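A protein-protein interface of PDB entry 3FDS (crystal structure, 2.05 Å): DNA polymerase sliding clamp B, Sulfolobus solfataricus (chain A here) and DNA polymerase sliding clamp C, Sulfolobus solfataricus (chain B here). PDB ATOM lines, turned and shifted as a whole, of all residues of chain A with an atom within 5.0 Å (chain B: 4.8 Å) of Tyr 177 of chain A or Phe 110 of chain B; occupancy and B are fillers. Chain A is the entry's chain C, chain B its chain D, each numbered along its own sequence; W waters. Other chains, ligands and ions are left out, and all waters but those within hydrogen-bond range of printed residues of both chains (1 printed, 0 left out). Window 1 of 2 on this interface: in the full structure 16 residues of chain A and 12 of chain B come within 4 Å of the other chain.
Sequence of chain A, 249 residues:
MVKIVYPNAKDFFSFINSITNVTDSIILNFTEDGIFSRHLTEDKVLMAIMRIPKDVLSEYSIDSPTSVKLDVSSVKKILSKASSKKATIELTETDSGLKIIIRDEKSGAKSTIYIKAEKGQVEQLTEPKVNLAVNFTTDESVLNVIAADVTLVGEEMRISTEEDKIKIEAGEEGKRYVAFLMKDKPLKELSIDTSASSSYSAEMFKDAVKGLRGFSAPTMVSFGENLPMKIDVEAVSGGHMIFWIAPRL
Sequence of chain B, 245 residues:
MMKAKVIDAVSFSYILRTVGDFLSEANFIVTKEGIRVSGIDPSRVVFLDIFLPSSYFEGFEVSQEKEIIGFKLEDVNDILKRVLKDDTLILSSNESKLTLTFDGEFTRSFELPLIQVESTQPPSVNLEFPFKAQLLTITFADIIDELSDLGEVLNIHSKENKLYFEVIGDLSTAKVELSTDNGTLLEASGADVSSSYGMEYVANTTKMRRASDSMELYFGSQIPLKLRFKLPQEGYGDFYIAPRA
Water W1 bridges O of Val 178 of chain A and OG of Ser 109 of chain B.
Ile 146 of chain A touches Phe 106 of chain B.
Asp 149 of chain A touches Phe 110 of chain B.
Leu 152 of chain A touches Arg 82 of chain B (CD2 to CG, 3.8 Å).
Phe 110 of chain B touches Val 153 of chain A.
Glu 111 of chain B touches Lys 175 of chain A.
Arg 176 of chain A touches Phe 110 of chain B.
OH of Tyr 177 of chain A touches CG of Arg 108 of chain B, at 3.6 Å.
CA of Tyr 177 of chain A touches O of Ser 109 of chain B (3.3 Å).
Tyr 177 of chain A touches Phe 110 of chain B.
O of Val 178 of chain A touches CA of Arg 108 of chain B (3.5 Å).
The backbone carbonyl oxygen of Leu 100 of chain B lies within hydrogen-bond range of the backbone NH of Phe 110 of chain B.
OD2 of Asp 149 of chain A is in hydrogen-bond range of OH of Tyr 177 of chain A, at 2.7 Å.
The backbone carbonyl oxygen (O) of Arg 108 of chain B sits at hydrogen-bond distance from the backbone NH (N) of Phe 102 of chain B.
NH2 of Arg 176 of chain A is in salt-bridge range of OE2 of Glu 169 of chain A (3.2 Å).
O of Ala 170 of chain A sits at hydrogen-bond distance from N of Tyr 177 of chain A, at 2.9 Å.
The backbone carbonyl oxygen (O) of Arg 82 of chain B lies within hydrogen-bond range of the guanidinium group (NH2) of Arg 108 of chain B (3.0 Å).
Of chain B, only Arg 108, Ser 109 and Phe 110 come within 4 Å of Tyr 177 of chain A.
Of the printed residues of chain A, Phe 110 of chain B touches Asp 149 (3.6 Å), Val 153 (3.7 Å), Arg 176 (3.3 Å) and Tyr 177 (3.5 Å).
Of the printed residues of chain B, Val 153 of chain A touches Phe 110.
Printed residues of chain A within 4 Å of Arg 108 of chain B: Asp 149, Tyr 177 and Val 178.
Of the printed residues of chain A, Glu 111 of chain B touches Lys 175 (3.4 Å) and Arg 176 (2.8 Å).
Ala 179 of chain A touches none of the printed residues of chain B.
Ala 170 of chain A touches none of the printed residues of chain B.
The nearest residue of chain B that does not touch Tyr 177 of chain A is Phe 106 of chain B (4.7 Å).
Of the 14 printed residues of chain A, 8 touch a printed residue of chain B.
Hydrophobic or aromatic side chains of chain A that line the printed part of chain B: Ile 146, Leu 152, Val 153 and Tyr 177.
Hydrophobic or aromatic side chains of chain B within 4 Å of the printed part of chain A: Phe 106 and Phe 110.
N of Val 178 of chain A sits at hydrogen-bond distance from O of Ser 109 of chain B, at 2.9 Å.
NH1 of Arg 108 of chain B is in salt-bridge range of OD1 of Asp 149 of chain A (3.1 Å).
The side-chain carboxylate (OE1) of Glu 111 of chain B lies within salt-bridge range of the guanidinium group (NE) of Arg 176 of chain A.
OD1 of Asp 149 of chain A is in salt-bridge range of NE of Arg 82 of chain B (2.7 Å).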
ATOM      1  N   ILE A 146      -9.206  26.148   6.237  1.00  0.00           N
ATOM      2  CA  ILE A 146      -9.459  25.804   4.826  1.00  0.00           C
ATOM      3  C   ILE A 146     -10.158  24.463   4.681  1.00  0.00           C
ATOM      4  O   ILE A 146     -11.161  24.351   3.973  1.00  0.00           O
ATOM      5  CB  ILE A 146      -8.135  25.722   3.999  1.00  0.00           C
ATOM      6  CG1 ILE A 146      -7.368  27.043   4.068  1.00  0.00           C
ATOM      7  CG2 ILE A 146      -8.421  25.341   2.534  1.00  0.00           C
ATOM      8  CD1 ILE A 146      -8.239  28.265   3.895  1.00  0.00           C
ATOM      9  N   ASP A 149     -13.650  24.584   6.027  1.00  0.00           N
ATOM     10  CA  ASP A 149     -14.496  25.363   5.113  1.00  0.00           C
ATOM     11  C   ASP A 149     -14.858  24.559   3.843  1.00  0.00           C
ATOM     12  O   ASP A 149     -16.023  24.538   3.457  1.00  0.00           O
ATOM     13  CB  ASP A 149     -13.798  26.632   4.639  1.00  0.00           C
ATOM     14  CG  ASP A 149     -13.593  27.674   5.752  1.00  0.00           C
ATOM     15  OD1 ASP A 149     -14.274  27.674   6.827  1.00  0.00           O
ATOM     16  OD2 ASP A 149     -12.756  28.526   5.481  1.00  0.00           O
ATOM     17  N   VAL A 150     -13.853  23.959   3.200  1.00  0.00           N
ATOM     18  CA  VAL A 150     -14.095  23.244   1.941  1.00  0.00           C
ATOM     19  C   VAL A 150     -15.008  22.061   2.140  1.00  0.00           C
ATOM     20  O   VAL A 150     -15.922  21.786   1.331  1.00  0.00           O
ATOM     21  CB  VAL A 150     -12.817  22.869   1.126  1.00  0.00           C
ATOM     22  CG1 VAL A 150     -12.069  24.149   0.706  1.00  0.00           C
ATOM     23  CG2 VAL A 150     -11.876  21.864   1.816  1.00  0.00           C
ATOM     24  N   LEU A 152     -17.208  21.601   4.471  1.00  0.00           N
ATOM     25  CA  LEU A 152     -18.597  22.031   4.707  1.00  0.00           C
ATOM     26  C   LEU A 152     -19.368  22.233   3.360  1.00  0.00           C
ATOM     27  O   LEU A 152     -20.585  22.040   3.263  1.00  0.00           O
ATOM     28  CB  LEU A 152     -18.588  23.432   5.388  1.00  0.00           C
ATOM     29  CG  LEU A 152     -19.937  24.070   5.657  1.00  0.00           C
ATOM     30  CD1 LEU A 152     -20.651  23.209   6.739  1.00  0.00           C
ATOM     31  CD2 LEU A 152     -19.913  25.599   6.007  1.00  0.00           C
ATOM     32  N   VAL A 153     -18.646  22.682   2.342  1.00  0.00           N
ATOM     33  CA  VAL A 153     -19.302  23.160   1.115  1.00  0.00           C
ATOM     34  C   VAL A 153     -19.260  22.137  -0.055  1.00  0.00           C
ATOM     35  O   VAL A 153     -20.176  22.063  -0.847  1.00  0.00           O
ATOM     36  CB  VAL A 153     -18.610  24.507   0.716  1.00  0.00           C
ATOM     37  CG1 VAL A 153     -18.916  24.856  -0.673  1.00  0.00           C
ATOM     38  CG2 VAL A 153     -19.095  25.648   1.732  1.00  0.00           C
ATOM     39  N   ILE A 168      -8.699  29.303  -3.404  1.00  0.00           N
ATOM     40  CA  ILE A 168      -9.256  27.994  -3.035  1.00  0.00           C
ATOM     41  C   ILE A 168     -10.740  28.091  -3.229  1.00  0.00           C
ATOM     42  O   ILE A 168     -11.355  29.045  -2.744  1.00  0.00           O
ATOM     43  CB  ILE A 168      -8.894  27.625  -1.591  1.00  0.00           C
ATOM     44  CG1 ILE A 168      -7.384  27.356  -1.545  1.00  0.00           C
ATOM     45  CG2 ILE A 168      -9.604  26.307  -1.147  1.00  0.00           C
ATOM     46  CD1 ILE A 168      -6.810  27.353  -0.231  1.00  0.00           C
ATOM     47  N   GLU A 169     -11.295  27.153  -4.008  1.00  0.00           N
ATOM     48  CA  GLU A 169     -12.705  27.124  -4.326  1.00  0.00           C
ATOM     49  C   GLU A 169     -13.298  25.730  -4.037  1.00  0.00           C
ATOM     50  O   GLU A 169     -12.616  24.690  -4.178  1.00  0.00           O
ATOM     51  CB  GLU A 169     -12.922  27.425  -5.805  1.00  0.00           C
ATOM     52  CG  GLU A 169     -12.744  28.870  -6.224  1.00  0.00           C
ATOM     53  CD  GLU A 169     -12.788  29.000  -7.737  1.00  0.00           C
ATOM     54  OE1 GLU A 169     -11.815  28.574  -8.395  1.00  0.00           O
ATOM     55  OE2 GLU A 169     -13.799  29.506  -8.270  1.00  0.00           O
ATOM     56  N   ALA A 170     -14.557  25.708  -3.643  1.00  0.00           N
ATOM     57  CA  ALA A 170     -15.285  24.430  -3.501  1.00  0.00           C
ATOM     58  C   ALA A 170     -16.721  24.788  -3.697  1.00  0.00           C
ATOM     59  O   ALA A 170     -17.092  25.938  -3.526  1.00  0.00           O
ATOM     60  CB  ALA A 170     -15.074  23.870  -2.107  1.00  0.00           C
ATOM     61  N   GLY A 171     -17.550  23.820  -4.087  1.00  0.00           N
ATOM     62  CA  GLY A 171     -18.949  24.078  -4.195  1.00  0.00           C
ATOM     63  C   GLY A 171     -19.771  22.958  -4.778  1.00  0.00           C
ATOM     64  O   GLY A 171     -19.272  22.044  -5.405  1.00  0.00           O
ATOM     65  N   LYS A 175     -23.933  26.470  -4.351  1.00  0.00           N
ATOM     66  CA  LYS A 175     -23.467  26.744  -2.979  1.00  0.00           C
ATOM     67  C   LYS A 175     -21.971  26.615  -2.877  1.00  0.00           C
ATOM     68  O   LYS A 175     -21.469  25.498  -2.828  1.00  0.00           O
ATOM     69  CB  LYS A 175     -24.139  25.775  -1.975  1.00  0.00           C
ATOM     70  CG  LYS A 175     -25.695  25.836  -1.951  1.00  0.00           C
ATOM     71  CD  LYS A 175     -26.231  25.021  -0.803  1.00  0.00           C
ATOM     72  CE  LYS A 175     -27.690  24.716  -0.981  1.00  0.00           C
ATOM     73  NZ  LYS A 175     -28.275  24.026   0.197  1.00  0.00           N
ATOM     74  N   ARG A 176     -21.267  27.739  -2.743  1.00  0.00           N
ATOM     75  CA  ARG A 176     -19.869  27.816  -3.086  1.00  0.00           C
ATOM     76  C   ARG A 176     -19.105  28.478  -1.971  1.00  0.00           C
ATOM     77  O   ARG A 176     -19.685  29.157  -1.110  1.00  0.00           O
ATOM     78  CB  ARG A 176     -19.665  28.691  -4.351  1.00  0.00           C
ATOM     79  CG  ARG A 176     -19.704  27.904  -5.649  1.00  0.00           C
ATOM     80  CD  ARG A 176     -19.692  28.814  -6.879  1.00  0.00           C
ATOM     81  NE  ARG A 176     -18.656  29.862  -6.870  1.00  0.00           N
ATOM     82  CZ  ARG A 176     -17.341  29.680  -7.096  1.00  0.00           C
ATOM     83  NH1 ARG A 176     -16.827  28.461  -7.323  1.00  0.00           N
ATOM     84  NH2 ARG A 176     -16.525  30.735  -7.087  1.00  0.00           N
ATOM     85  N   TYR A 177     -17.796  28.283  -2.016  1.00  0.00           N
ATOM     86  CA  TYR A 177     -16.839  28.876  -1.109  1.00  0.00           C
ATOM     87  C   TYR A 177     -15.675  29.349  -1.951  1.00  0.00           C
ATOM     88  O   TYR A 177     -15.272  28.638  -2.885  1.00  0.00           O
ATOM     89  CB  TYR A 177     -16.253  27.764  -0.216  1.00  0.00           C
ATOM     90  CG  TYR A 177     -15.058  28.143   0.640  1.00  0.00           C
ATOM     91  CD1 TYR A 177     -15.196  28.973   1.746  1.00  0.00           C
ATOM     92  CD2 TYR A 177     -13.787  27.613   0.364  1.00  0.00           C
ATOM     93  CE1 TYR A 177     -14.085  29.292   2.539  1.00  0.00           C
ATOM     94  CE2 TYR A 177     -12.707  27.905   1.129  1.00  0.00           C
ATOM     95  CZ  TYR A 177     -12.853  28.719   2.243  1.00  0.00           C
ATOM     96  OH  TYR A 177     -11.763  28.954   3.058  1.00  0.00           O
ATOM     97  N   VAL A 178     -15.132  30.533  -1.636  1.00  0.00           N
ATOM     98  CA  VAL A 178     -13.858  30.982  -2.236  1.00  0.00           C
ATOM     99  C   VAL A 178     -12.978  31.726  -1.233  1.00  0.00           C
ATOM    100  O   VAL A 178     -13.438  32.666  -0.590  1.00  0.00           O
ATOM    101  CB  VAL A 178     -14.081  31.855  -3.525  1.00  0.00           C
ATOM    102  CG1 VAL A 178     -14.870  33.139  -3.212  1.00  0.00           C
ATOM    103  CG2 VAL A 178     -12.747  32.209  -4.177  1.00  0.00           C
ATOM    104  N   ALA A 179     -11.717  31.311  -1.109  1.00  0.00           N
ATOM    105  CA  ALA A 179     -10.768  31.988  -0.245  1.00  0.00           C
ATOM    106  C   ALA A 179      -9.567  32.417  -1.045  1.00  0.00           C
ATOM    107  O   ALA A 179      -9.183  31.744  -1.996  1.00  0.00           O
ATOM    108  CB  ALA A 179     -10.305  31.012   0.934  1.00  0.00           C
ATOM    109  N   ILE B  79     -22.762  28.262   7.895  1.00  0.00           N
ATOM    110  CA  ILE B  79     -21.743  29.182   7.462  1.00  0.00           C
ATOM    111  C   ILE B  79     -21.320  30.122   8.591  1.00  0.00           C
ATOM    112  O   ILE B  79     -20.113  30.359   8.769  1.00  0.00           O
ATOM    113  CB  ILE B  79     -22.227  30.002   6.199  1.00  0.00           C
ATOM    114  CG1 ILE B  79     -22.380  29.094   4.968  1.00  0.00           C
ATOM    115  CG2 ILE B  79     -21.265  31.159   5.850  1.00  0.00           C
ATOM    116  CD1 ILE B  79     -23.119  29.884   3.797  1.00  0.00           C
ATOM    117  N   ARG B  82     -18.638  29.283  10.939  1.00  0.00           N
ATOM    118  CA  ARG B  82     -17.283  29.277  10.363  1.00  0.00           C
ATOM    119  C   ARG B  82     -16.515  30.573  10.667  1.00  0.00           C
ATOM    120  O   ARG B  82     -15.327  30.702  10.317  1.00  0.00           O
ATOM    121  CB  ARG B  82     -17.316  29.003   8.866  1.00  0.00           C
ATOM    122  CG  ARG B  82     -17.883  27.563   8.496  1.00  0.00           C
ATOM    123  CD  ARG B  82     -17.022  26.333   9.050  1.00  0.00           C
ATOM    124  NE  ARG B  82     -15.611  26.578   8.879  1.00  0.00           N
ATOM    125  CZ  ARG B  82     -14.691  26.544   9.844  1.00  0.00           C
ATOM    126  NH1 ARG B  82     -13.407  26.852   9.550  1.00  0.00           N
ATOM    127  NH2 ARG B  82     -15.024  26.148  11.086  1.00  0.00           N
ATOM    128  N   LEU B  98     -26.952  35.210  -2.245  1.00  0.00           N
ATOM    129  CA  LEU B  98     -26.563  35.842  -1.021  1.00  0.00           C
ATOM    130  C   LEU B  98     -25.120  35.430  -0.765  1.00  0.00           C
ATOM    131  O   LEU B  98     -24.787  34.241  -0.867  1.00  0.00           O
ATOM    132  CB  LEU B  98     -27.440  35.310   0.112  1.00  0.00           C
ATOM    133  CG  LEU B  98     -27.039  35.567   1.567  1.00  0.00           C
ATOM    134  CD1 LEU B  98     -27.204  37.057   1.893  1.00  0.00           C
ATOM    135  CD2 LEU B  98     -27.925  34.699   2.431  1.00  0.00           C
ATOM    136  N   THR B  99     -24.279  36.389  -0.378  1.00  0.00           N
ATOM    137  CA  THR B  99     -22.884  36.112  -0.019  1.00  0.00           C
ATOM    138  C   THR B  99     -22.591  36.535   1.439  1.00  0.00           C
ATOM    139  O   THR B  99     -22.964  37.643   1.867  1.00  0.00           O
ATOM    140  CB  THR B  99     -21.933  36.829  -0.988  1.00  0.00           C
ATOM    141  OG1 THR B  99     -22.223  36.406  -2.314  1.00  0.00           O
ATOM    142  CG2 THR B  99     -20.482  36.499  -0.734  1.00  0.00           C
ATOM    143  N   LEU B 100     -21.954  35.628   2.177  1.00  0.00           N
ATOM    144  CA  LEU B 100     -21.396  35.940   3.513  1.00  0.00           C
ATOM    145  C   LEU B 100     -19.880  35.865   3.421  1.00  0.00           C
ATOM    146  O   LEU B 100     -19.305  34.819   3.109  1.00  0.00           O
ATOM    147  CB  LEU B 100     -21.935  34.972   4.567  1.00  0.00           C
ATOM    148  CG  LEU B 100     -23.458  34.807   4.722  1.00  0.00           C
ATOM    149  CD1 LEU B 100     -23.790  33.877   5.847  1.00  0.00           C
ATOM    150  CD2 LEU B 100     -24.080  36.089   5.059  1.00  0.00           C
ATOM    151  N   PHE B 102     -16.190  36.681   5.323  1.00  0.00           N
ATOM    152  CA  PHE B 102     -15.404  36.852   6.548  1.00  0.00           C
ATOM    153  C   PHE B 102     -14.057  37.449   6.156  1.00  0.00           C
ATOM    154  O   PHE B 102     -13.278  36.837   5.430  1.00  0.00           O
ATOM    155  CB  PHE B 102     -15.198  35.509   7.254  1.00  0.00           C
ATOM    156  CG  PHE B 102     -16.481  34.828   7.676  1.00  0.00           C
ATOM    157  CD1 PHE B 102     -16.813  33.578   7.170  1.00  0.00           C
ATOM    158  CD2 PHE B 102     -17.347  35.429   8.591  1.00  0.00           C
ATOM    159  CE1 PHE B 102     -17.996  32.950   7.524  1.00  0.00           C
ATOM    160  CE2 PHE B 102     -18.567  34.788   8.965  1.00  0.00           C
ATOM    161  CZ  PHE B 102     -18.873  33.534   8.410  1.00  0.00           C
ATOM    162  N   PHE B 106      -7.310  36.352   6.641  1.00  0.00           N
ATOM    163  CA  PHE B 106      -7.436  36.367   5.170  1.00  0.00           C
ATOM    164  C   PHE B 106      -8.928  36.368   4.812  1.00  0.00           C
ATOM    165  O   PHE B 106      -9.749  36.326   5.698  1.00  0.00           O
ATOM    166  CB  PHE B 106      -6.712  35.180   4.524  1.00  0.00           C
ATOM    167  CG  PHE B 106      -7.175  33.828   5.001  1.00  0.00           C
ATOM    168  CD1 PHE B 106      -6.730  33.318   6.217  1.00  0.00           C
ATOM    169  CD2 PHE B 106      -8.029  33.036   4.214  1.00  0.00           C
ATOM    170  CE1 PHE B 106      -7.134  32.058   6.664  1.00  0.00           C
ATOM    171  CE2 PHE B 106      -8.404  31.763   4.628  1.00  0.00           C
ATOM    172  CZ  PHE B 106      -7.971  31.281   5.880  1.00  0.00           C
ATOM    173  N   ARG B 108     -12.506  35.039   3.021  1.00  0.00           N
ATOM    174  CA  ARG B 108     -13.235  33.803   2.738  1.00  0.00           C
ATOM    175  C   ARG B 108     -14.691  34.199   2.503  1.00  0.00           C
ATOM    176  O   ARG B 108     -15.266  34.815   3.383  1.00  0.00           O
ATOM    177  CB  ARG B 108     -13.185  32.828   3.999  1.00  0.00           C
ATOM    178  CG  ARG B 108     -11.782  32.331   4.432  1.00  0.00           C
ATOM    179  CD  ARG B 108     -11.722  31.573   5.816  1.00  0.00           C
ATOM    180  NE  ARG B 108     -12.386  32.303   6.904  1.00  0.00           N
ATOM    181  CZ  ARG B 108     -13.319  31.840   7.729  1.00  0.00           C
ATOM    182  NH1 ARG B 108     -13.757  30.579   7.689  1.00  0.00           N
ATOM    183  NH2 ARG B 108     -13.818  32.658   8.626  1.00  0.00           N
ATOM    184  N   SER B 109     -15.302  33.832   1.377  1.00  0.00           N
ATOM    185  CA  SER B 109     -16.767  34.026   1.175  1.00  0.00           C
ATOM    186  C   SER B 109     -17.463  32.742   0.890  1.00  0.00           C
ATOM    187  O   SER B 109     -16.919  31.837   0.235  1.00  0.00           O
ATOM    188  CB  SER B 109     -17.115  34.909  -0.043  1.00  0.00           C
ATOM    189  OG  SER B 109     -16.067  35.722  -0.358  1.00  0.00           O
ATOM    190  N   PHE B 110     -18.701  32.707   1.360  1.00  0.00           N
ATOM    191  CA  PHE B 110     -19.601  31.593   1.109  1.00  0.00           C
ATOM    192  C   PHE B 110     -20.798  32.171   0.386  1.00  0.00           C
ATOM    193  O   PHE B 110     -21.346  33.189   0.806  1.00  0.00           O
ATOM    194  CB  PHE B 110     -20.038  30.976   2.424  1.00  0.00           C
ATOM    195  CG  PHE B 110     -18.934  30.384   3.242  1.00  0.00           C
ATOM    196  CD1 PHE B 110     -18.069  31.205   4.018  1.00  0.00           C
ATOM    197  CD2 PHE B 110     -18.767  28.999   3.269  1.00  0.00           C
ATOM    198  CE1 PHE B 110     -17.048  30.622   4.808  1.00  0.00           C
ATOM    199  CE2 PHE B 110     -17.779  28.380   4.055  1.00  0.00           C
ATOM    200  CZ  PHE B 110     -16.910  29.189   4.842  1.00  0.00           C
ATOM    201  N   GLU B 111     -21.190  31.542  -0.721  1.00  0.00           N
ATOM    202  CA  GLU B 111     -22.356  32.007  -1.499  1.00  0.00           C
ATOM    203  C   GLU B 111     -23.451  30.985  -1.405  1.00  0.00           C
ATOM    204  O   GLU B 111     -23.178  29.775  -1.423  1.00  0.00           O
ATOM    205  CB  GLU B 111     -21.990  32.102  -2.976  1.00  0.00           C
ATOM    206  CG  GLU B 111     -20.847  33.037  -3.225  1.00  0.00           C
ATOM    207  CD  GLU B 111     -20.289  32.931  -4.657  1.00  0.00           C
ATOM    208  OE1 GLU B 111     -20.904  32.278  -5.542  1.00  0.00           O
ATOM    209  OE2 GLU B 111     -19.215  33.524  -4.870  1.00  0.00           O
ATOM    210  N   LEU B 112     -24.677  31.471  -1.337  1.00  0.00           N
ATOM    211  CA  LEU B 112     -25.903  30.656  -1.422  1.00  0.00           C
ATOM    212  C   LEU B 112     -26.806  31.266  -2.472  1.00  0.00           C
ATOM    213  O   LEU B 112     -27.166  32.429  -2.324  1.00  0.00           O
ATOM    214  CB  LEU B 112     -26.632  30.711  -0.085  1.00  0.00           C
ATOM    215  CG  LEU B 112     -25.864  30.096   1.123  1.00  0.00           C
ATOM    216  CD1 LEU B 112     -26.578  30.503   2.408  1.00  0.00           C
ATOM    217  CD2 LEU B 112     -25.730  28.560   1.035  1.00  0.00           C
HETATM  218  O   HOH W   1     -13.294  35.465  -0.884  1.00  0.00           O
